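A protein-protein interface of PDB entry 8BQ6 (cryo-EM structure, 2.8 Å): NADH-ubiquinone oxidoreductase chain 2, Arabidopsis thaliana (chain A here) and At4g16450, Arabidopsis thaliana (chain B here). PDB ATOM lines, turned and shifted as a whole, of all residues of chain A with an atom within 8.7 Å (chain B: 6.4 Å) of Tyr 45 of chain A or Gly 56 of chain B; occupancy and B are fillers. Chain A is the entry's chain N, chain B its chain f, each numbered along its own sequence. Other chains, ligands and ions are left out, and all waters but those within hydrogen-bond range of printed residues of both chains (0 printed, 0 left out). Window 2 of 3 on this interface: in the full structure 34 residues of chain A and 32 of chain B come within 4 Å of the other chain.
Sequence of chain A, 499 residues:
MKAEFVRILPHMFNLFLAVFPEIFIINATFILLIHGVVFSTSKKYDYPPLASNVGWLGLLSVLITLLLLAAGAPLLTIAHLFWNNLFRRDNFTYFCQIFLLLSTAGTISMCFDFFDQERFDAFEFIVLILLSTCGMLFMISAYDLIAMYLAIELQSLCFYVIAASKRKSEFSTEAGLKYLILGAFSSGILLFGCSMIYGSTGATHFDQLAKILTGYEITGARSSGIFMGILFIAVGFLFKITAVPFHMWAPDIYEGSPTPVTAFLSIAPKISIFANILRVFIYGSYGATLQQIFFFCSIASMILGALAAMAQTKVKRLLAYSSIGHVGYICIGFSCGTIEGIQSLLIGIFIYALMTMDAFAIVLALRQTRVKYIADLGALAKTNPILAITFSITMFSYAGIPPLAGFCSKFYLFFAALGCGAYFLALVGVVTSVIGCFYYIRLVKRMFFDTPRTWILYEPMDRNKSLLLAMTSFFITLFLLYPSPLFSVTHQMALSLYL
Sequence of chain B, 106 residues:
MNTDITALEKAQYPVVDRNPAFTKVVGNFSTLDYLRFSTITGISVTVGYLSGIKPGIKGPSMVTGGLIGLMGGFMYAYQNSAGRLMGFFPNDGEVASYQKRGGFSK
N of Lys 58 of chain B lies within hydrogen-bond range of O of Gly 52 of chain B (3.2 Å). The backbone carbonyl oxygen (O) of Gly 52 of chain B lies within hydrogen-bond range of the backbone NH (N) of Ile 57 of chain B (2.9 Å).
Hydrophobic or aromatic side chains of chain B within 4 Å of the printed part of chain A: Pro 55, Ile 57 and Pro 60. Of the 14 printed residues of chain A, 6 touch a printed residue of chain B.
Among the printed residues, pairs that only touch across the chains: Phe 39 of chain A with Pro 60 of chain B (3.4 Å), Tyr 45 of chain A with Gly 56 of chain B (3.8 Å), Tyr 45 of chain A with Ile 57 of chain B (3.6 Å), Pro 48 of chain A with Pro 55 of chain B (3.3 Å), Pro 49 of chain A with Pro 55 of chain B (3.7 Å), Leu 50 of chain A with Pro 55 of chain B (3.8 Å), Leu 50 of chain A with Ile 57 of chain B (3.7 Å), Asn 53 of chain A with Gly 52 of chain B (3.9 Å) and Asn 53 of chain A with Ile 57 of chain B (3.5 Å).
Of the printed residues of chain B, Tyr 45 of chain A touches Gly 56 and Ile 57. Of the printed residues of chain A, Gly 56 of chain B touches Tyr 45. Printed residues of chain A within 4 Å of Pro 55 of chain B: Pro 48, Pro 49 and Leu 50. Of the printed residues of chain A, Pro 60 of chain B touches Phe 39 (3.4 Å). Printed residues of chain B within 4 Å of Asn 53 of chain A: Gly 52 and Ile 57. Of the printed residues of chain B, Pro 48 of chain A touches Pro 55 (3.3 Å). Of the printed residues of chain B, Leu 50 of chain A touches Pro 55 and Ile 57. Of the printed residues of chain A, Ile 57 of chain B touches Tyr 45, Leu 50 and Asn 53. The nearest printed residue of chain B that does not touch Leu 50 of chain A is Gly 56 of chain B (6.8 Å).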
ATOM      1  N   VAL A  38       1.864 -22.488  18.955  1.00  0.00           N
ATOM      2  CA  VAL A  38       2.208 -21.431  19.900  1.00  0.00           C
ATOM      3  C   VAL A  38       3.338 -21.864  20.824  1.00  0.00           C
ATOM      4  O   VAL A  38       4.294 -21.110  21.042  1.00  0.00           O
ATOM      5  CB  VAL A  38       0.965 -20.988  20.688  1.00  0.00           C
ATOM      6  CG1 VAL A  38       1.369 -20.244  21.938  1.00  0.00           C
ATOM      7  CG2 VAL A  38       0.115 -20.080  19.827  1.00  0.00           C
ATOM      8  N   PHE A  39       3.265 -23.068  21.389  1.00  0.00           N
ATOM      9  CA  PHE A  39       4.287 -23.370  22.383  1.00  0.00           C
ATOM     10  C   PHE A  39       5.503 -24.074  21.817  1.00  0.00           C
ATOM     11  O   PHE A  39       6.520 -24.159  22.508  1.00  0.00           O
ATOM     12  CB  PHE A  39       3.691 -24.168  23.536  1.00  0.00           C
ATOM     13  CG  PHE A  39       2.761 -23.360  24.353  1.00  0.00           C
ATOM     14  CD1 PHE A  39       3.247 -22.394  25.209  1.00  0.00           C
ATOM     15  CD2 PHE A  39       1.400 -23.504  24.213  1.00  0.00           C
ATOM     16  CE1 PHE A  39       2.393 -21.618  25.936  1.00  0.00           C
ATOM     17  CE2 PHE A  39       0.543 -22.730  24.939  1.00  0.00           C
ATOM     18  CZ  PHE A  39       1.041 -21.784  25.800  1.00  0.00           C
ATOM     19  N   SER A  40       5.453 -24.537  20.573  1.00  0.00           N
ATOM     20  CA  SER A  40       6.665 -25.077  19.978  1.00  0.00           C
ATOM     21  C   SER A  40       7.619 -23.973  19.536  1.00  0.00           C
ATOM     22  O   SER A  40       8.828 -24.207  19.445  1.00  0.00           O
ATOM     23  CB  SER A  40       6.313 -25.974  18.803  1.00  0.00           C
ATOM     24  OG  SER A  40       6.355 -25.231  17.604  1.00  0.00           O
ATOM     25  N   THR A  41       7.106 -22.778  19.245  1.00  0.00           N
ATOM     26  CA  THR A  41       7.947 -21.674  18.806  1.00  0.00           C
ATOM     27  C   THR A  41       8.459 -20.846  19.972  1.00  0.00           C
ATOM     28  O   THR A  41       9.242 -19.915  19.763  1.00  0.00           O
ATOM     29  CB  THR A  41       7.184 -20.762  17.841  1.00  0.00           C
ATOM     30  OG1 THR A  41       5.849 -20.565  18.315  1.00  0.00           O
ATOM     31  CG2 THR A  41       7.092 -21.413  16.484  1.00  0.00           C
ATOM     32  N   SER A  42       8.040 -21.173  21.188  1.00  0.00           N
ATOM     33  CA  SER A  42       8.304 -20.340  22.353  1.00  0.00           C
ATOM     34  C   SER A  42       9.764 -20.479  22.757  1.00  0.00           C
ATOM     35  O   SER A  42      10.220 -21.572  23.107  1.00  0.00           O
ATOM     36  CB  SER A  42       7.382 -20.733  23.501  1.00  0.00           C
ATOM     37  OG  SER A  42       7.520 -19.837  24.586  1.00  0.00           O
ATOM     38  N   LYS A  43      10.494 -19.366  22.700  1.00  0.00           N
ATOM     39  CA  LYS A  43      11.850 -19.327  23.233  1.00  0.00           C
ATOM     40  C   LYS A  43      11.846 -19.535  24.739  1.00  0.00           C
ATOM     41  O   LYS A  43      12.787 -20.100  25.307  1.00  0.00           O
ATOM     42  CB  LYS A  43      12.495 -17.988  22.886  1.00  0.00           C
ATOM     43  CG  LYS A  43      13.925 -17.837  23.346  1.00  0.00           C
ATOM     44  CD  LYS A  43      14.622 -16.726  22.582  1.00  0.00           C
ATOM     45  CE  LYS A  43      14.014 -15.358  22.872  1.00  0.00           C
ATOM     46  NZ  LYS A  43      14.197 -14.929  24.292  1.00  0.00           N
ATOM     47  N   LYS A  44      10.787 -19.073  25.401  1.00  0.00           N
ATOM     48  CA  LYS A  44      10.734 -19.111  26.855  1.00  0.00           C
ATOM     49  C   LYS A  44      10.759 -20.544  27.375  1.00  0.00           C
ATOM     50  O   LYS A  44      11.445 -20.849  28.357  1.00  0.00           O
ATOM     51  CB  LYS A  44       9.491 -18.368  27.327  1.00  0.00           C
ATOM     52  CG  LYS A  44       9.224 -18.490  28.788  1.00  0.00           C
ATOM     53  CD  LYS A  44       7.863 -17.947  29.113  1.00  0.00           C
ATOM     54  CE  LYS A  44       7.589 -18.079  30.590  1.00  0.00           C
ATOM     55  NZ  LYS A  44       6.226 -17.604  30.920  1.00  0.00           N
ATOM     56  N   TYR A  45      10.029 -21.440  26.721  1.00  0.00           N
ATOM     57  CA  TYR A  45      10.046 -22.851  27.074  1.00  0.00           C
ATOM     58  C   TYR A  45      11.083 -23.640  26.290  1.00  0.00           C
ATOM     59  O   TYR A  45      11.048 -24.875  26.312  1.00  0.00           O
ATOM     60  CB  TYR A  45       8.657 -23.454  26.887  1.00  0.00           C
ATOM     61  CG  TYR A  45       7.612 -22.742  27.706  1.00  0.00           C
ATOM     62  CD1 TYR A  45       7.574 -22.887  29.082  1.00  0.00           C
ATOM     63  CD2 TYR A  45       6.676 -21.920  27.109  1.00  0.00           C
ATOM     64  CE1 TYR A  45       6.627 -22.239  29.839  1.00  0.00           C
ATOM     65  CE2 TYR A  45       5.726 -21.269  27.859  1.00  0.00           C
ATOM     66  CZ  TYR A  45       5.707 -21.431  29.221  1.00  0.00           C
ATOM     67  OH  TYR A  45       4.760 -20.782  29.968  1.00  0.00           O
ATOM     68  N   ASP A  46      12.001 -22.951  25.611  1.00  0.00           N
ATOM     69  CA  ASP A  46      13.127 -23.566  24.907  1.00  0.00           C
ATOM     70  C   ASP A  46      12.651 -24.487  23.786  1.00  0.00           C
ATOM     71  O   ASP A  46      13.184 -25.581  23.596  1.00  0.00           O
ATOM     72  CB  ASP A  46      14.050 -24.313  25.876  1.00  0.00           C
ATOM     73  CG  ASP A  46      15.368 -24.713  25.237  1.00  0.00           C
ATOM     74  OD1 ASP A  46      15.876 -23.949  24.392  1.00  0.00           O
ATOM     75  OD2 ASP A  46      15.896 -25.791  25.577  1.00  0.00           O
ATOM     76  N   TYR A  47      11.645 -24.042  23.040  1.00  0.00           N
ATOM     77  CA  TYR A  47      11.119 -24.775  21.894  1.00  0.00           C
ATOM     78  C   TYR A  47      10.849 -26.245  22.220  1.00  0.00           C
ATOM     79  O   TYR A  47      11.471 -27.139  21.642  1.00  0.00           O
ATOM     80  CB  TYR A  47      12.064 -24.656  20.708  1.00  0.00           C
ATOM     81  CG  TYR A  47      12.604 -23.269  20.532  1.00  0.00           C
ATOM     82  CD1 TYR A  47      11.901 -22.334  19.797  1.00  0.00           C
ATOM     83  CD2 TYR A  47      13.811 -22.890  21.100  1.00  0.00           C
ATOM     84  CE1 TYR A  47      12.374 -21.073  19.630  1.00  0.00           C
ATOM     85  CE2 TYR A  47      14.293 -21.621  20.938  1.00  0.00           C
ATOM     86  CZ  TYR A  47      13.568 -20.718  20.199  1.00  0.00           C
ATOM     87  OH  TYR A  47      14.029 -19.441  20.018  1.00  0.00           O
ATOM     88  N   PRO A  48       9.934 -26.523  23.142  1.00  0.00           N
ATOM     89  CA  PRO A  48       9.742 -27.888  23.606  1.00  0.00           C
ATOM     90  C   PRO A  48       9.189 -28.771  22.504  1.00  0.00           C
ATOM     91  O   PRO A  48       8.326 -28.343  21.724  1.00  0.00           O
ATOM     92  CB  PRO A  48       8.730 -27.728  24.746  1.00  0.00           C
ATOM     93  CG  PRO A  48       7.999 -26.495  24.418  1.00  0.00           C
ATOM     94  CD  PRO A  48       8.975 -25.590  23.754  1.00  0.00           C
ATOM     95  N   PRO A  49       9.669 -30.007  22.398  1.00  0.00           N
ATOM     96  CA  PRO A  49       9.006 -30.973  21.518  1.00  0.00           C
ATOM     97  C   PRO A  49       7.610 -31.262  22.041  1.00  0.00           C
ATOM     98  O   PRO A  49       7.430 -31.630  23.202  1.00  0.00           O
ATOM     99  CB  PRO A  49       9.902 -32.210  21.610  1.00  0.00           C
ATOM    100  CG  PRO A  49      11.208 -31.707  22.025  1.00  0.00           C
ATOM    101  CD  PRO A  49      10.967 -30.501  22.882  1.00  0.00           C
ATOM    102  N   LEU A  50       6.613 -31.102  21.175  1.00  0.00           N
ATOM    103  CA  LEU A  50       5.227 -31.245  21.596  1.00  0.00           C
ATOM    104  C   LEU A  50       4.526 -32.442  20.973  1.00  0.00           C
ATOM    105  O   LEU A  50       3.300 -32.549  21.087  1.00  0.00           O
ATOM    106  CB  LEU A  50       4.450 -29.964  21.289  1.00  0.00           C
ATOM    107  CG  LEU A  50       4.915 -28.806  22.166  1.00  0.00           C
ATOM    108  CD1 LEU A  50       4.235 -27.509  21.790  1.00  0.00           C
ATOM    109  CD2 LEU A  50       4.667 -29.148  23.617  1.00  0.00           C
ATOM    110  N   ASN A  53       2.907 -34.553  23.810  1.00  0.00           N
ATOM    111  CA  ASN A  53       1.881 -33.787  24.511  1.00  0.00           C
ATOM    112  C   ASN A  53       0.613 -33.683  23.671  1.00  0.00           C
ATOM    113  O   ASN A  53      -0.494 -34.010  24.129  1.00  0.00           O
ATOM    114  CB  ASN A  53       2.427 -32.398  24.839  1.00  0.00           C
ATOM    115  CG  ASN A  53       1.392 -31.497  25.456  1.00  0.00           C
ATOM    116  OD1 ASN A  53       1.355 -30.304  25.181  1.00  0.00           O
ATOM    117  ND2 ASN A  53       0.571 -32.053  26.333  1.00  0.00           N
ATOM    118  N   GLY B  52       1.836 -32.462  29.969  1.00  0.00           N
ATOM    119  CA  GLY B  52       2.615 -31.246  29.841  1.00  0.00           C
ATOM    120  C   GLY B  52       3.890 -31.185  30.650  1.00  0.00           C
ATOM    121  O   GLY B  52       4.667 -30.242  30.485  1.00  0.00           O
ATOM    122  N   ILE B  53       4.133 -32.171  31.514  1.00  0.00           N
ATOM    123  CA  ILE B  53       5.287 -32.124  32.407  1.00  0.00           C
ATOM    124  C   ILE B  53       6.591 -32.247  31.629  1.00  0.00           C
ATOM    125  O   ILE B  53       7.533 -31.475  31.844  1.00  0.00           O
ATOM    126  CB  ILE B  53       5.170 -33.217  33.482  1.00  0.00           C
ATOM    127  CG1 ILE B  53       4.052 -32.868  34.461  1.00  0.00           C
ATOM    128  CG2 ILE B  53       6.497 -33.405  34.195  1.00  0.00           C
ATOM    129  CD1 ILE B  53       3.623 -34.014  35.312  1.00  0.00           C
ATOM    130  N   LYS B  54       6.679 -33.228  30.731  1.00  0.00           N
ATOM    131  CA  LYS B  54       7.938 -33.443  30.019  1.00  0.00           C
ATOM    132  C   LYS B  54       8.351 -32.246  29.170  1.00  0.00           C
ATOM    133  O   LYS B  54       9.514 -31.821  29.274  1.00  0.00           O
ATOM    134  CB  LYS B  54       7.865 -34.725  29.182  1.00  0.00           C
ATOM    135  CG  LYS B  54       9.118 -34.929  28.339  1.00  0.00           C
ATOM    136  CD  LYS B  54       9.355 -36.376  27.933  1.00  0.00           C
ATOM    137  CE  LYS B  54       8.297 -36.889  26.971  1.00  0.00           C
ATOM    138  NZ  LYS B  54       7.642 -35.805  26.191  1.00  0.00           N
ATOM    139  N   PRO B  55       7.488 -31.650  28.339  1.00  0.00           N
ATOM    140  CA  PRO B  55       7.911 -30.446  27.610  1.00  0.00           C
ATOM    141  C   PRO B  55       8.055 -29.218  28.490  1.00  0.00           C
ATOM    142  O   PRO B  55       8.571 -28.200  28.016  1.00  0.00           O
ATOM    143  CB  PRO B  55       6.803 -30.256  26.571  1.00  0.00           C
ATOM    144  CG  PRO B  55       5.637 -30.899  27.164  1.00  0.00           C
ATOM    145  CD  PRO B  55       6.142 -32.078  27.918  1.00  0.00           C
ATOM    146  N   GLY B  56       7.605 -29.268  29.740  1.00  0.00           N
ATOM    147  CA  GLY B  56       7.738 -28.137  30.636  1.00  0.00           C
ATOM    148  C   GLY B  56       6.613 -27.130  30.600  1.00  0.00           C
ATOM    149  O   GLY B  56       6.798 -26.001  31.065  1.00  0.00           O
ATOM    150  N   ILE B  57       5.453 -27.493  30.063  1.00  0.00           N
ATOM    151  CA  ILE B  57       4.347 -26.558  29.886  1.00  0.00           C
ATOM    152  C   ILE B  57       3.088 -27.057  30.583  1.00  0.00           C
ATOM    153  O   ILE B  57       1.992 -26.974  30.021  1.00  0.00           O
ATOM    154  CB  ILE B  57       4.085 -26.283  28.396  1.00  0.00           C
ATOM    155  CG1 ILE B  57       3.964 -27.594  27.625  1.00  0.00           C
ATOM    156  CG2 ILE B  57       5.178 -25.406  27.821  1.00  0.00           C
ATOM    157  CD1 ILE B  57       3.017 -27.513  26.475  1.00  0.00           C
ATOM    158  N   LYS B  58       3.239 -27.645  31.773  1.00  0.00           N
ATOM    159  CA  LYS B  58       2.104 -28.299  32.423  1.00  0.00           C
ATOM    160  C   LYS B  58       0.911 -27.364  32.613  1.00  0.00           C
ATOM    161  O   LYS B  58      -0.234 -27.804  32.488  1.00  0.00           O
ATOM    162  CB  LYS B  58       2.535 -28.895  33.761  1.00  0.00           C
ATOM    163  CG  LYS B  58       2.986 -27.893  34.783  1.00  0.00           C
ATOM    164  CD  LYS B  58       3.819 -28.572  35.839  1.00  0.00           C
ATOM    165  CE  LYS B  58       3.814 -27.779  37.121  1.00  0.00           C
ATOM    166  NZ  LYS B  58       4.456 -28.554  38.204  1.00  0.00           N
ATOM    167  N   GLY B  59       1.145 -26.083  32.892  1.00  0.00           N
ATOM    168  CA  GLY B  59       0.068 -25.133  33.067  1.00  0.00           C
ATOM    169  C   GLY B  59      -0.691 -24.803  31.791  1.00  0.00           C
ATOM    170  O   GLY B  59      -1.927 -24.887  31.731  1.00  0.00           O
ATOM    171  N   PRO B  60       0.030 -24.365  30.756  1.00  0.00           N
ATOM    172  CA  PRO B  60      -0.631 -24.168  29.455  1.00  0.00           C
ATOM    173  C   PRO B  60      -1.263 -25.434  28.902  1.00  0.00           C
ATOM    174  O   PRO B  60      -2.354 -25.377  28.318  1.00  0.00           O
ATOM    175  CB  PRO B  60       0.508 -23.658  28.569  1.00  0.00           C
ATOM    176  CG  PRO B  60       1.436 -22.983  29.517  1.00  0.00           C
ATOM    177  CD  PRO B  60       1.393 -23.807  30.768  1.00  0.00           C
